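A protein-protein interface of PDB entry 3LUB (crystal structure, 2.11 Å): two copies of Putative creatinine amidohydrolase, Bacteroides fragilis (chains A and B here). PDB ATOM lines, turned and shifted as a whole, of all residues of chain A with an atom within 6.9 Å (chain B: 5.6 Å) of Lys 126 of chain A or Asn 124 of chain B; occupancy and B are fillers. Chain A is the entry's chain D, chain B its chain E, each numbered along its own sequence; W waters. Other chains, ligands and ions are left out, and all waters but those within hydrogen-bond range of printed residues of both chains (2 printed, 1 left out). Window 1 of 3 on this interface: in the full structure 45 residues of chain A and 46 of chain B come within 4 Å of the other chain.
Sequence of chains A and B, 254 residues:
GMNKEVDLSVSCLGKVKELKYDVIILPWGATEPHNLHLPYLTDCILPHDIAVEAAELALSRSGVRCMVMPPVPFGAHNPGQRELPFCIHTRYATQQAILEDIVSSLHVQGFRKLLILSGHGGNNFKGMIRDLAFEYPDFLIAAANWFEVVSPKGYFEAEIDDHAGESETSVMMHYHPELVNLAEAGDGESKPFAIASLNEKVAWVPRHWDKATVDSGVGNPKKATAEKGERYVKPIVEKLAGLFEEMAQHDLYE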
ATOM      1  N   TYR A  92     -18.652 -31.129   0.561  1.00  0.00           N
ATOM      2  CA  TYR A  92     -18.249 -29.709   0.782  1.00  0.00           C
ATOM      3  C   TYR A  92     -17.226 -29.559   1.897  1.00  0.00           C
ATOM      4  O   TYR A  92     -16.314 -28.744   1.798  1.00  0.00           O
ATOM      5  CB  TYR A  92     -19.463 -28.792   1.127  1.00  0.00           C
ATOM      6  CG  TYR A  92     -19.209 -27.286   0.968  1.00  0.00           C
ATOM      7  CD1 TYR A  92     -18.595 -26.511   1.972  1.00  0.00           C
ATOM      8  CD2 TYR A  92     -19.597 -26.631  -0.194  1.00  0.00           C
ATOM      9  CE1 TYR A  92     -18.390 -25.110   1.790  1.00  0.00           C
ATOM     10  CE2 TYR A  92     -19.386 -25.285  -0.374  1.00  0.00           C
ATOM     11  CZ  TYR A  92     -18.796 -24.519   0.621  1.00  0.00           C
ATOM     12  OH  TYR A  92     -18.630 -23.180   0.323  1.00  0.00           O
ATOM     13  N   ASN A 124     -18.350 -24.905  -5.758  1.00  0.00           N
ATOM     14  CA  ASN A 124     -18.841 -23.638  -5.250  1.00  0.00           C
ATOM     15  C   ASN A 124     -17.985 -23.277  -4.056  1.00  0.00           C
ATOM     16  O   ASN A 124     -17.933 -24.044  -3.104  1.00  0.00           O
ATOM     17  CB  ASN A 124     -20.293 -23.804  -4.783  1.00  0.00           C
ATOM     18  CG  ASN A 124     -21.277 -23.867  -5.921  1.00  0.00           C
ATOM     19  OD1 ASN A 124     -21.501 -22.862  -6.593  1.00  0.00           O
ATOM     20  ND2 ASN A 124     -21.906 -25.048  -6.128  1.00  0.00           N
ATOM     21  N   PHE A 125     -17.329 -22.129  -4.125  1.00  0.00           N
ATOM     22  CA  PHE A 125     -16.312 -21.694  -3.143  1.00  0.00           C
ATOM     23  C   PHE A 125     -16.665 -20.447  -2.288  1.00  0.00           C
ATOM     24  O   PHE A 125     -15.893 -20.087  -1.411  1.00  0.00           O
ATOM     25  CB  PHE A 125     -14.979 -21.427  -3.873  1.00  0.00           C
ATOM     26  CG  PHE A 125     -14.457 -22.635  -4.612  1.00  0.00           C
ATOM     27  CD1 PHE A 125     -13.856 -23.661  -3.922  1.00  0.00           C
ATOM     28  CD2 PHE A 125     -14.606 -22.760  -5.986  1.00  0.00           C
ATOM     29  CE1 PHE A 125     -13.423 -24.788  -4.548  1.00  0.00           C
ATOM     30  CE2 PHE A 125     -14.136 -23.898  -6.636  1.00  0.00           C
ATOM     31  CZ  PHE A 125     -13.538 -24.907  -5.918  1.00  0.00           C
ATOM     32  N   LYS A 126     -17.831 -19.836  -2.512  1.00  0.00           N
ATOM     33  CA  LYS A 126     -18.190 -18.572  -1.878  1.00  0.00           C
ATOM     34  C   LYS A 126     -18.327 -18.707  -0.382  1.00  0.00           C
ATOM     35  O   LYS A 126     -17.819 -17.869   0.345  1.00  0.00           O
ATOM     36  CB  LYS A 126     -19.469 -17.950  -2.485  1.00  0.00           C
ATOM     37  CG  LYS A 126     -19.335 -17.586  -3.925  1.00  0.00           C
ATOM     38  CD  LYS A 126     -20.529 -16.852  -4.450  1.00  0.00           C
ATOM     39  CE  LYS A 126     -20.411 -16.671  -5.964  1.00  0.00           C
ATOM     40  NZ  LYS A 126     -21.655 -16.070  -6.445  1.00  0.00           N
ATOM     41  N   GLY A 127     -18.963 -19.779   0.079  1.00  0.00           N
ATOM     42  CA  GLY A 127     -19.041 -20.065   1.513  1.00  0.00           C
ATOM     43  C   GLY A 127     -17.676 -20.247   2.180  1.00  0.00           C
ATOM     44  O   GLY A 127     -17.396 -19.713   3.279  1.00  0.00           O
ATOM     45  N   MET A 128     -16.817 -21.027   1.531  1.00  0.00           N
ATOM     46  CA  MET A 128     -15.478 -21.290   2.079  1.00  0.00           C
ATOM     47  C   MET A 128     -14.696 -19.991   2.152  1.00  0.00           C
ATOM     48  O   MET A 128     -13.993 -19.714   3.138  1.00  0.00           O
ATOM     49  CB  MET A 128     -14.688 -22.250   1.165  1.00  0.00           C
ATOM     50  CG  MET A 128     -15.246 -23.671   1.099  1.00  0.00           C
ATOM     51  SD  MET A 128     -14.217 -24.724  -0.134  1.00  0.00           S
ATOM     52  CE  MET A 128     -15.685 -25.778  -0.968  1.00  0.00           C
ATOM     53  N   ILE A 129     -14.782 -19.227   1.085  1.00  0.00           N
ATOM     54  CA  ILE A 129     -14.099 -17.953   1.002  1.00  0.00           C
ATOM     55  C   ILE A 129     -14.615 -16.995   2.091  1.00  0.00           C
ATOM     56  O   ILE A 129     -13.820 -16.301   2.713  1.00  0.00           O
ATOM     57  CB  ILE A 129     -14.213 -17.366  -0.401  1.00  0.00           C
ATOM     58  CG1 ILE A 129     -13.301 -18.097  -1.375  1.00  0.00           C
ATOM     59  CG2 ILE A 129     -13.839 -15.868  -0.450  1.00  0.00           C
ATOM     60  CD1 ILE A 129     -13.666 -17.744  -2.877  1.00  0.00           C
ATOM     61  N   ARG A 130     -15.917 -16.978   2.350  1.00  0.00           N
ATOM     62  CA  ARG A 130     -16.478 -16.143   3.421  1.00  0.00           C
ATOM     63  C   ARG A 130     -15.878 -16.511   4.761  1.00  0.00           C
ATOM     64  O   ARG A 130     -15.420 -15.651   5.517  1.00  0.00           O
ATOM     65  CB  ARG A 130     -18.012 -16.249   3.482  1.00  0.00           C
ATOM     66  CG  ARG A 130     -18.704 -15.461   2.383  1.00  0.00           C
ATOM     67  CD  ARG A 130     -20.165 -15.334   2.580  1.00  0.00           C
ATOM     68  NE  ARG A 130     -20.681 -14.309   1.685  1.00  0.00           N
ATOM     69  CZ  ARG A 130     -21.184 -14.536   0.485  1.00  0.00           C
ATOM     70  NH1 ARG A 130     -21.316 -15.774   0.022  1.00  0.00           N
ATOM     71  NH2 ARG A 130     -21.585 -13.516  -0.248  1.00  0.00           N
ATOM     72  N   ASP A 131     -15.876 -17.797   5.048  1.00  0.00           N
ATOM     73  CA  ASP A 131     -15.399 -18.263   6.329  1.00  0.00           C
ATOM     74  C   ASP A 131     -13.907 -18.038   6.536  1.00  0.00           C
ATOM     75  O   ASP A 131     -13.473 -17.703   7.651  1.00  0.00           O
ATOM     76  CB  ASP A 131     -15.781 -19.724   6.514  1.00  0.00           C
ATOM     77  CG  ASP A 131     -17.292 -19.930   6.704  1.00  0.00           C
ATOM     78  OD1 ASP A 131     -18.033 -18.980   7.029  1.00  0.00           O
ATOM     79  OD2 ASP A 131     -17.722 -21.086   6.553  1.00  0.00           O
ATOM     80  N   ALA A 143     -12.386 -16.385  -6.645  1.00  0.00           N
ATOM     81  CA  ALA A 143     -12.753 -17.607  -7.361  1.00  0.00           C
ATOM     82  C   ALA A 143     -13.317 -17.265  -8.732  1.00  0.00           C
ATOM     83  O   ALA A 143     -14.099 -16.322  -8.840  1.00  0.00           O
ATOM     84  CB  ALA A 143     -13.780 -18.367  -6.608  1.00  0.00           C
ATOM     85  N   TYR B  92     -20.557 -21.979   7.151  1.00  0.00           N
ATOM     86  CA  TYR B  92     -21.185 -22.936   6.268  1.00  0.00           C
ATOM     87  C   TYR B  92     -21.467 -24.236   6.989  1.00  0.00           C
ATOM     88  O   TYR B  92     -22.561 -24.781   6.846  1.00  0.00           O
ATOM     89  CB  TYR B  92     -20.286 -23.228   5.036  1.00  0.00           C
ATOM     90  CG  TYR B  92     -21.000 -24.002   3.935  1.00  0.00           C
ATOM     91  CD1 TYR B  92     -21.180 -25.380   4.004  1.00  0.00           C
ATOM     92  CD2 TYR B  92     -21.492 -23.332   2.829  1.00  0.00           C
ATOM     93  CE1 TYR B  92     -21.862 -26.069   2.974  1.00  0.00           C
ATOM     94  CE2 TYR B  92     -22.162 -23.988   1.821  1.00  0.00           C
ATOM     95  CZ  TYR B  92     -22.339 -25.354   1.876  1.00  0.00           C
ATOM     96  OH  TYR B  92     -23.022 -25.934   0.812  1.00  0.00           O
ATOM     97  N   GLN B  95     -24.499 -23.912   9.218  1.00  0.00           N
ATOM     98  CA  GLN B  95     -25.691 -23.977   8.384  1.00  0.00           C
ATOM     99  C   GLN B  95     -26.002 -25.422   7.919  1.00  0.00           C
ATOM    100  O   GLN B  95     -27.174 -25.861   7.911  1.00  0.00           O
ATOM    101  CB  GLN B  95     -25.565 -23.071   7.188  1.00  0.00           C
ATOM    102  CG  GLN B  95     -25.345 -21.591   7.478  1.00  0.00           C
ATOM    103  CD  GLN B  95     -25.390 -20.798   6.212  1.00  0.00           C
ATOM    104  OE1 GLN B  95     -24.664 -21.098   5.254  1.00  0.00           O
ATOM    105  NE2 GLN B  95     -26.248 -19.761   6.181  1.00  0.00           N
ATOM    106  N   GLY B 121     -28.903 -13.433  -0.111  1.00  0.00           N
ATOM    107  CA  GLY B 121     -28.065 -13.821  -1.239  1.00  0.00           C
ATOM    108  C   GLY B 121     -26.719 -14.434  -0.891  1.00  0.00           C
ATOM    109  O   GLY B 121     -26.146 -15.125  -1.708  1.00  0.00           O
ATOM    110  N   GLY B 122     -26.225 -14.153   0.316  1.00  0.00           N
ATOM    111  CA  GLY B 122     -25.028 -14.761   0.869  1.00  0.00           C
ATOM    112  C   GLY B 122     -25.185 -16.238   1.192  1.00  0.00           C
ATOM    113  O   GLY B 122     -24.194 -16.931   1.364  1.00  0.00           O
ATOM    114  N   ASN B 123     -26.420 -16.728   1.289  1.00  0.00           N
ATOM    115  CA  ASN B 123     -26.645 -18.149   1.554  1.00  0.00           C
ATOM    116  C   ASN B 123     -26.517 -18.926   0.235  1.00  0.00           C
ATOM    117  O   ASN B 123     -27.043 -18.519  -0.791  1.00  0.00           O
ATOM    118  CB  ASN B 123     -28.016 -18.440   2.182  1.00  0.00           C
ATOM    119  CG  ASN B 123     -28.208 -17.807   3.555  1.00  0.00           C
ATOM    120  OD1 ASN B 123     -27.253 -17.552   4.283  1.00  0.00           O
ATOM    121  ND2 ASN B 123     -29.462 -17.557   3.904  1.00  0.00           N
ATOM    122  N   ASN B 124     -25.800 -20.032   0.302  1.00  0.00           N
ATOM    123  CA  ASN B 124     -25.626 -20.960  -0.805  1.00  0.00           C
ATOM    124  C   ASN B 124     -25.907 -22.353  -0.293  1.00  0.00           C
ATOM    125  O   ASN B 124     -25.318 -22.768   0.688  1.00  0.00           O
ATOM    126  CB  ASN B 124     -24.191 -20.873  -1.279  1.00  0.00           C
ATOM    127  CG  ASN B 124     -23.932 -19.629  -2.088  1.00  0.00           C
ATOM    128  OD1 ASN B 124     -24.407 -19.521  -3.236  1.00  0.00           O
ATOM    129  ND2 ASN B 124     -23.177 -18.667  -1.503  1.00  0.00           N
ATOM    130  N   PHE B 125     -26.790 -23.069  -0.961  1.00  0.00           N
ATOM    131  CA  PHE B 125     -27.238 -24.353  -0.493  1.00  0.00           C
ATOM    132  C   PHE B 125     -26.933 -25.522  -1.455  1.00  0.00           C
ATOM    133  O   PHE B 125     -27.248 -26.652  -1.140  1.00  0.00           O
ATOM    134  CB  PHE B 125     -28.746 -24.285  -0.253  1.00  0.00           C
ATOM    135  CG  PHE B 125     -29.143 -23.305   0.805  1.00  0.00           C
ATOM    136  CD1 PHE B 125     -28.971 -23.618   2.149  1.00  0.00           C
ATOM    137  CD2 PHE B 125     -29.690 -22.092   0.468  1.00  0.00           C
ATOM    138  CE1 PHE B 125     -29.311 -22.723   3.118  1.00  0.00           C
ATOM    139  CE2 PHE B 125     -30.049 -21.200   1.442  1.00  0.00           C
ATOM    140  CZ  PHE B 125     -29.873 -21.511   2.759  1.00  0.00           C
ATOM    141  N   LYS B 126     -26.279 -25.264  -2.584  1.00  0.00           N
ATOM    142  CA  LYS B 126     -26.094 -26.309  -3.595  1.00  0.00           C
ATOM    143  C   LYS B 126     -25.219 -27.435  -3.091  1.00  0.00           C
ATOM    144  O   LYS B 126     -25.559 -28.595  -3.248  1.00  0.00           O
ATOM    145  CB  LYS B 126     -25.507 -25.732  -4.854  1.00  0.00           C
ATOM    146  CG  LYS B 126     -26.368 -24.677  -5.497  1.00  0.00           C
ATOM    147  CD  LYS B 126     -25.927 -24.451  -6.919  1.00  0.00           C
ATOM    148  CE  LYS B 126     -26.718 -23.308  -7.574  1.00  0.00           C
ATOM    149  NZ  LYS B 126     -26.452 -23.239  -8.989  1.00  0.00           N
ATOM    150  N   GLY B 127     -24.097 -27.099  -2.484  1.00  0.00           N
ATOM    151  CA  GLY B 127     -23.245 -28.088  -1.884  1.00  0.00           C
ATOM    152  C   GLY B 127     -23.911 -28.930  -0.813  1.00  0.00           C
ATOM    153  O   GLY B 127     -23.723 -30.150  -0.787  1.00  0.00           O
ATOM    154  N   MET B 128     -24.682 -28.286   0.077  1.00  0.00           N
ATOM    155  CA  MET B 128     -25.426 -28.985   1.123  1.00  0.00           C
ATOM    156  C   MET B 128     -26.423 -29.936   0.505  1.00  0.00           C
ATOM    157  O   MET B 128     -26.609 -31.063   0.972  1.00  0.00           O
ATOM    158  CB  MET B 128     -26.223 -28.004   2.011  1.00  0.00           C
ATOM    159  CG  MET B 128     -25.480 -26.906   2.553  1.00  0.00           C
ATOM    160  SD  MET B 128     -26.458 -25.896   3.922  1.00  0.00           S
ATOM    161  CE  MET B 128     -25.232 -24.376   3.782  1.00  0.00           C
ATOM    162  N   TRP B 204     -14.764 -13.592  -8.576  1.00  0.00           N
ATOM    163  CA  TRP B 204     -15.584 -13.146  -7.463  1.00  0.00           C
ATOM    164  C   TRP B 204     -14.753 -13.050  -6.195  1.00  0.00           C
ATOM    165  O   TRP B 204     -13.923 -13.930  -5.887  1.00  0.00           O
ATOM    166  CB  TRP B 204     -16.750 -14.116  -7.240  1.00  0.00           C
ATOM    167  CG  TRP B 204     -17.619 -13.799  -6.051  1.00  0.00           C
ATOM    168  CD1 TRP B 204     -18.748 -13.034  -6.041  1.00  0.00           C
ATOM    169  CD2 TRP B 204     -17.469 -14.297  -4.708  1.00  0.00           C
ATOM    170  NE1 TRP B 204     -19.278 -12.987  -4.791  1.00  0.00           N
ATOM    171  CE2 TRP B 204     -18.519 -13.744  -3.946  1.00  0.00           C
ATOM    172  CE3 TRP B 204     -16.539 -15.144  -4.076  1.00  0.00           C
ATOM    173  CZ2 TRP B 204     -18.679 -14.011  -2.588  1.00  0.00           C
ATOM    174  CZ3 TRP B 204     -16.691 -15.399  -2.732  1.00  0.00           C
ATOM    175  CH2 TRP B 204     -17.754 -14.842  -1.997  1.00  0.00           C
HETATM  176  O   HOH W   1     -23.328 -15.545  -2.105  1.00  0.00           O
HETATM  177  O   HOH W   2     -17.709 -23.739   7.449  1.00  0.00           O
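The backbone NH (N) of Tyr 92 of chain B sits at hydrogen-bond distance from the side-chain carboxylate (OD2) of Asp 131 of chain A, at 3.0 Å. O of Ala 143 of chain A sits at hydrogen-bond distance from N of Trp 204 of chain B, at 2.8 Å. NH1 of Arg 130 of chain A is in hydrogen-bond range of O of Gly 122 of chain B (3.4 Å).
The backbone NH (N) of Met 128 of chain A sits at hydrogen-bond distance from the side-chain hydroxyl (OH) of Tyr 92 of chain A (3.1 Å). The side-chain hydroxyl (OH) of Tyr 92 of chain B is in hydrogen-bond range of the backbone NH (N) of Met 128 of chain B, at 3.0 Å. The side-chain hydroxyl of Tyr 92 of chain A lies close to the backbone NH of Gly 127 of chain A.
Among the printed residues, pairs that only touch across the chains: Tyr 92 of chain A with Tyr 92 of chain B, Asn 124 of chain A with Lys 126 of chain B, Lys 126 of chain A with Asn 124 of chain B, Lys 126 of chain A with Trp 204 of chain B, Ile 129 of chain A with Trp 204 of chain B, Arg 130 of chain A with Asn 124 of chain B and Arg 130 of chain A with Trp 204 of chain B.
Of the printed residues of chain B, Asn 124 of chain A touches Lys 126. Of the printed residues of chain B, Arg 130 of chain A touches Gly 122, Asn 124 and Trp 204. Gln 95 of chain B touches none of the printed residues of chain A. Of chain A, only Lys 126 (3.9 Å) and Arg 130 (3.8 Å) come within 4 Å of Asn 124 of chain B. Of the printed residues of chain A, Lys 126 of chain B touches Asn 124 (3.9 Å). The nearest printed residue of chain B that does not touch Lys 126 of chain A is Gly 122 of chain B (6.2 Å). The nearest printed residue of chain B that does not touch Tyr 92 of chain A is Gly 127 of chain B (4.3 Å).
Of the 11 printed residues of chain B, 5 touch a printed residue of chain A. Hydrophobic or aromatic side chains of chain B that line the printed part of chain A: Tyr 92 and Trp 204. Of the 10 printed residues of chain A, 7 touch a printed residue of chain B. Printed residues of chain A that touch a printed residue of chain B: Tyr 92, Asn 124, Lys 126, Ile 129, Arg 130, Asp 131 and Ala 143. Among the printed residues, 10 pairs touch across the chains. Among the printed residues, no Asp or Glu carboxylate lies within 4 Å of a Lys or Arg side-chain nitrogen of the other chain.
Tyr 92 of chain A touches its own counterpart, Tyr 92 of chain B. Asn 124 of chain A touches Lys 126 of chain B, and with the chains exchanged Lys 126 of chain A touches Asn 124 of chain B. Of the 10 pairs that touch across the chains among the printed residues, 3 have their exchanged pair printed and touching as well.
Water W2 bridges OD2 of Asp 131 of chain A (2.8 Å) and N of Tyr 92 of chain B (3.4 Å). Water W1 lies within hydrogen-bond range of the backbone carbonyl oxygen (O) of Gly 121 of chain B (2.9 Å), the guanidinium group (NH1) of Arg 130 of chain A (2.9 Å) and the side-chain amide nitrogen (ND2) of Asn 124 of chain B (3.2 Å).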
